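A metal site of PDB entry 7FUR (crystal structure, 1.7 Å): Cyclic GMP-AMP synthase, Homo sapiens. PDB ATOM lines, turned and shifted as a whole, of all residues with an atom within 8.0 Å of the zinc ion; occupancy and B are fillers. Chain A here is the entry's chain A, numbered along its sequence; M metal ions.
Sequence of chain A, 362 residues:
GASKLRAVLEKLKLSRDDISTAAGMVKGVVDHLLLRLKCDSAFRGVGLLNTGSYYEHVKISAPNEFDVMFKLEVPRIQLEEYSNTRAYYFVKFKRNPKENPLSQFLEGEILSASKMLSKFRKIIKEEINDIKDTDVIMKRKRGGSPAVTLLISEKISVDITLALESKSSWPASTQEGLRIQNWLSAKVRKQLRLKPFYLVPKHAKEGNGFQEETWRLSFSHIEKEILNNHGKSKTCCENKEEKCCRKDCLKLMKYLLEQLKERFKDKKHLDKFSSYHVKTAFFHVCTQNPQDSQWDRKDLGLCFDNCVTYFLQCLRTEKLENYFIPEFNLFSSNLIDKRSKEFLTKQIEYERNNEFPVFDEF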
ATOM      1  N   LEU A 227      16.332   7.051  29.599  1.00  0.00           N
ATOM      2  CA  LEU A 227      16.407   8.441  29.134  1.00  0.00           C
ATOM      3  C   LEU A 227      15.534   8.684  27.916  1.00  0.00           C
ATOM      4  O   LEU A 227      14.928   9.747  27.780  1.00  0.00           O
ATOM      5  CB  LEU A 227      17.869   8.811  28.832  1.00  0.00           C
ATOM      6  CG  LEU A 227      18.583   9.306  30.097  1.00  0.00           C
ATOM      7  CD1 LEU A 227      20.078   9.383  29.857  1.00  0.00           C
ATOM      8  CD2 LEU A 227      18.038  10.686  30.452  1.00  0.00           C
ATOM      9  N   ASN A 229      12.772   7.124  27.085  1.00  0.00           N
ATOM     10  CA  ASN A 229      11.398   6.718  27.363  1.00  0.00           C
ATOM     11  C   ASN A 229      11.185   7.018  28.844  1.00  0.00           C
ATOM     12  O   ASN A 229      11.061   6.148  29.722  1.00  0.00           O
ATOM     13  CB  ASN A 229      11.148   5.236  27.028  1.00  0.00           C
ATOM     14  CG  ASN A 229       9.676   4.855  27.108  1.00  0.00           C
ATOM     15  OD1 ASN A 229       8.801   5.700  27.345  1.00  0.00           O
ATOM     16  ND2 ASN A 229       9.394   3.574  26.896  1.00  0.00           N
ATOM     17  N   HIS A 230      11.171   8.302  29.165  1.00  0.00           N
ATOM     18  CA  HIS A 230      11.479   8.777  30.493  1.00  0.00           C
ATOM     19  C   HIS A 230      10.294   9.319  31.271  1.00  0.00           C
ATOM     20  O   HIS A 230      10.493   9.829  32.370  1.00  0.00           O
ATOM     21  CB  HIS A 230      12.494   9.908  30.394  1.00  0.00           C
ATOM     22  CG  HIS A 230      11.974  11.062  29.598  1.00  0.00           C
ATOM     23  ND1 HIS A 230      12.478  11.405  28.356  1.00  0.00           N
ATOM     24  CD2 HIS A 230      10.950  11.922  29.848  1.00  0.00           C
ATOM     25  CE1 HIS A 230      11.806  12.439  27.887  1.00  0.00           C
ATOM     26  NE2 HIS A 230      10.867  12.777  28.767  1.00  0.00           N
ATOM     27  N   GLY A 231       9.098   9.349  30.683  1.00  0.00           N
ATOM     28  CA  GLY A 231       7.977   9.924  31.399  1.00  0.00           C
ATOM     29  C   GLY A 231       7.189   8.882  32.167  1.00  0.00           C
ATOM     30  O   GLY A 231       7.248   7.680  31.894  1.00  0.00           O
ATOM     31  N   LYS A 232       6.436   9.354  33.166  1.00  0.00           N
ATOM     32  CA  LYS A 232       5.365   8.541  33.714  1.00  0.00           C
ATOM     33  C   LYS A 232       4.303   8.295  32.641  1.00  0.00           C
ATOM     34  O   LYS A 232       3.840   7.173  32.447  1.00  0.00           O
ATOM     35  CB  LYS A 232       4.737   9.212  34.935  1.00  0.00           C
ATOM     36  CG  LYS A 232       3.469   8.476  35.413  1.00  0.00           C
ATOM     37  CD  LYS A 232       2.966   8.959  36.780  1.00  0.00           C
ATOM     38  CE  LYS A 232       3.968   8.642  37.898  1.00  0.00           C
ATOM     39  NZ  LYS A 232       4.184   7.187  38.017  1.00  0.00           N
ATOM     40  N   SER A 233       3.942   9.337  31.911  1.00  0.00           N
ATOM     41  CA  SER A 233       3.067   9.175  30.755  1.00  0.00           C
ATOM     42  C   SER A 233       3.834   8.576  29.590  1.00  0.00           C
ATOM     43  O   SER A 233       4.978   8.988  29.292  1.00  0.00           O
ATOM     44  CB  SER A 233       2.456  10.496  30.329  1.00  0.00           C
ATOM     45  OG  SER A 233       1.819  10.327  29.077  1.00  0.00           O
ATOM     46  N   THR A 235       3.223   9.124  26.648  1.00  0.00           N
ATOM     47  CA  THR A 235       3.328  10.165  25.638  1.00  0.00           C
ATOM     48  C   THR A 235       4.085  11.402  26.125  1.00  0.00           C
ATOM     49  O   THR A 235       3.973  12.462  25.518  1.00  0.00           O
ATOM     50  CB  THR A 235       1.936  10.582  25.132  1.00  0.00           C
ATOM     51  OG1 THR A 235       1.037  10.702  26.238  1.00  0.00           O
ATOM     52  CG2 THR A 235       1.387   9.572  24.151  1.00  0.00           C
ATOM     53  N   CYS A 236       4.869  11.266  27.197  1.00  0.00           N
ATOM     54  CA  CYS A 236       5.716  12.372  27.624  1.00  0.00           C
ATOM     55  C   CYS A 236       6.639  12.788  26.480  1.00  0.00           C
ATOM     56  O   CYS A 236       7.263  11.947  25.820  1.00  0.00           O
ATOM     57  CB  CYS A 236       6.557  11.980  28.841  1.00  0.00           C
ATOM     58  SG  CYS A 236       7.370  13.375  29.671  1.00  0.00           S
ATOM     59  N   CYS A 237       6.663  14.087  26.206  1.00  0.00           N
ATOM     60  CA  CYS A 237       7.443  14.696  25.139  1.00  0.00           C
ATOM     61  C   CYS A 237       7.028  14.259  23.730  1.00  0.00           C
ATOM     62  O   CYS A 237       7.795  14.448  22.789  1.00  0.00           O
ATOM     63  CB  CYS A 237       8.944  14.450  25.368  1.00  0.00           C
ATOM     64  SG  CYS A 237       9.614  15.420  26.731  1.00  0.00           S
ATOM     65  N   GLU A 238       5.811  13.709  23.547  1.00  0.00           N
ATOM     66  CA  GLU A 238       5.311  13.361  22.209  1.00  0.00           C
ATOM     67  C   GLU A 238       4.280  14.347  21.693  1.00  0.00           C
ATOM     68  O   GLU A 238       3.805  14.193  20.562  1.00  0.00           O
ATOM     69  CB  GLU A 238       4.702  11.958  22.186  1.00  0.00           C
ATOM     70  CG  GLU A 238       5.736  10.816  22.276  1.00  0.00           C
ATOM     71  CD  GLU A 238       5.148   9.471  21.833  1.00  0.00           C
ATOM     72  OE1 GLU A 238       3.915   9.400  21.600  1.00  0.00           O
ATOM     73  OE2 GLU A 238       5.920   8.487  21.716  1.00  0.00           O
ATOM     74  N   GLU A 242       2.737  17.892  26.723  1.00  0.00           N
ATOM     75  CA  GLU A 242       3.510  17.022  27.604  1.00  0.00           C
ATOM     76  C   GLU A 242       5.006  17.200  27.369  1.00  0.00           C
ATOM     77  O   GLU A 242       5.775  16.246  27.265  1.00  0.00           O
ATOM     78  CB  GLU A 242       3.117  15.556  27.414  1.00  0.00           C
ATOM     79  CG  GLU A 242       1.667  15.225  27.755  1.00  0.00           C
ATOM     80  CD  GLU A 242       1.392  13.718  27.692  1.00  0.00           C
ATOM     81  OE1 GLU A 242       1.934  12.967  28.532  1.00  0.00           O
ATOM     82  OE2 GLU A 242       0.656  13.287  26.783  1.00  0.00           O
ATOM     83  N   LYS A 243       5.446  18.453  27.327  1.00  0.00           N
ATOM     84  CA  LYS A 243       6.867  18.751  27.192  1.00  0.00           C
ATOM     85  C   LYS A 243       7.446  18.911  28.594  1.00  0.00           C
ATOM     86  O   LYS A 243       7.233  19.941  29.241  1.00  0.00           O
ATOM     87  CB  LYS A 243       7.077  20.009  26.368  1.00  0.00           C
ATOM     88  CG  LYS A 243       6.579  19.886  24.943  1.00  0.00           C
ATOM     89  CD  LYS A 243       7.524  19.061  24.095  1.00  0.00           C
ATOM     90  CE  LYS A 243       7.034  18.995  22.671  1.00  0.00           C
ATOM     91  NZ  LYS A 243       8.055  18.401  21.762  1.00  0.00           N
ATOM     92  N   CYS A 244       8.151  17.891  29.074  1.00  0.00           N
ATOM     93  CA  CYS A 244       8.839  17.976  30.354  1.00  0.00           C
ATOM     94  C   CYS A 244      10.247  18.537  30.142  1.00  0.00           C
ATOM     95  O   CYS A 244      10.732  18.680  29.015  1.00  0.00           O
ATOM     96  CB  CYS A 244       8.907  16.611  31.025  1.00  0.00           C
ATOM     97  SG  CYS A 244      10.175  15.447  30.382  1.00  0.00           S
ATOM     98  N   CYS A 245      10.924  18.849  31.237  1.00  0.00           N
ATOM     99  CA  CYS A 245      12.266  19.393  31.155  1.00  0.00           C
ATOM    100  C   CYS A 245      13.307  18.443  31.741  1.00  0.00           C
ATOM    101  O   CYS A 245      14.355  18.889  32.197  1.00  0.00           O
ATOM    102  CB  CYS A 245      12.329  20.756  31.822  1.00  0.00           C
ATOM    103  SG  CYS A 245      12.060  20.743  33.598  1.00  0.00           S
ATOM    104  N   ARG A 246      13.039  17.142  31.736  1.00  0.00           N
ATOM    105  CA  ARG A 246      13.995  16.211  32.331  1.00  0.00           C
ATOM    106  C   ARG A 246      15.336  16.243  31.581  1.00  0.00           C
ATOM    107  O   ARG A 246      16.399  16.372  32.199  1.00  0.00           O
ATOM    108  CB  ARG A 246      13.423  14.795  32.329  1.00  0.00           C
ATOM    109  CG  ARG A 246      12.287  14.568  33.314  1.00  0.00           C
ATOM    110  CD  ARG A 246      11.971  13.067  33.342  1.00  0.00           C
ATOM    111  NE  ARG A 246      10.949  12.655  34.303  1.00  0.00           N
ATOM    112  CZ  ARG A 246       9.649  12.764  34.063  1.00  0.00           C
ATOM    113  NH1 ARG A 246       8.752  12.339  34.951  1.00  0.00           N
ATOM    114  NH2 ARG A 246       9.240  13.298  32.927  1.00  0.00           N
ATOM    115  N   LYS A 247      15.304  16.093  30.260  1.00  0.00           N
ATOM    116  CA  LYS A 247      16.577  16.047  29.553  1.00  0.00           C
ATOM    117  C   LYS A 247      17.300  17.388  29.638  1.00  0.00           C
ATOM    118  O   LYS A 247      18.534  17.431  29.750  1.00  0.00           O
ATOM    119  CB  LYS A 247      16.368  15.632  28.101  1.00  0.00           C
ATOM    120  CG  LYS A 247      16.065  14.157  27.992  1.00  0.00           C
ATOM    121  CD  LYS A 247      16.227  13.658  26.560  1.00  0.00           C
ATOM    122  CE  LYS A 247      16.237  12.139  26.547  1.00  0.00           C
ATOM    123  NZ  LYS A 247      16.394  11.552  25.208  1.00  0.00           N
ATOM    124  N   ASP A 292       5.266  13.562  35.905  1.00  0.00           N
ATOM    125  CA  ASP A 292       5.676  14.455  34.830  1.00  0.00           C
ATOM    126  C   ASP A 292       5.397  15.910  35.191  1.00  0.00           C
ATOM    127  O   ASP A 292       6.128  16.817  34.773  1.00  0.00           O
ATOM    128  CB  ASP A 292       4.981  14.083  33.524  1.00  0.00           C
ATOM    129  CG  ASP A 292       5.344  12.686  33.025  1.00  0.00           C
ATOM    130  OD1 ASP A 292       6.385  12.136  33.431  1.00  0.00           O
ATOM    131  OD2 ASP A 292       4.557  12.141  32.227  1.00  0.00           O
ATOM    132  N   TRP A 295       8.058  18.047  36.411  1.00  0.00           N
ATOM    133  CA  TRP A 295       9.078  18.364  35.432  1.00  0.00           C
ATOM    134  C   TRP A 295       8.501  19.220  34.315  1.00  0.00           C
ATOM    135  O   TRP A 295       8.942  19.128  33.166  1.00  0.00           O
ATOM    136  CB  TRP A 295       9.684  17.079  34.864  1.00  0.00           C
ATOM    137  CG  TRP A 295      10.380  16.265  35.894  1.00  0.00           C
ATOM    138  CD1 TRP A 295       9.850  15.262  36.653  1.00  0.00           C
ATOM    139  CD2 TRP A 295      11.755  16.386  36.306  1.00  0.00           C
ATOM    140  NE1 TRP A 295      10.805  14.736  37.489  1.00  0.00           N
ATOM    141  CE2 TRP A 295      11.987  15.407  37.286  1.00  0.00           C
ATOM    142  CE3 TRP A 295      12.820  17.202  35.900  1.00  0.00           C
ATOM    143  CZ2 TRP A 295      13.237  15.229  37.905  1.00  0.00           C
ATOM    144  CZ3 TRP A 295      14.069  17.030  36.505  1.00  0.00           C
ATOM    145  CH2 TRP A 295      14.257  16.054  37.499  1.00  0.00           C
HETATM  146 ZN    ZN M   1       9.348  14.168  28.697  1.00  0.00          ZN
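O of His 230 lies within hydrogen-bond range of NE of Arg 246 (3.5 Å).
The backbone carbonyl oxygen of Leu 227 lies within hydrogen-bond range of a ring nitrogen (ND1) of His 230, 3.0 Å away.
The guanidinium group of Arg 246 lies close to the side-chain sulfur of Cys 244, at 3.5 Å.
The guanidinium group (NH2) of Arg 246 lies close to the side-chain sulfur (SG) of Cys 236 (3.8 Å).
O of Glu 242 is in hydrogen-bond range of N of Cys 237, at 2.6 Å.
The zinc ion is bound by NE2 of His 230 (2.1 Å), SG of Cys 244 (2.3 Å), SG of Cys 236 (2.3 Å) and SG of Cys 237 (2.3 Å).
The zinc ion has four donor atoms within binding distance.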
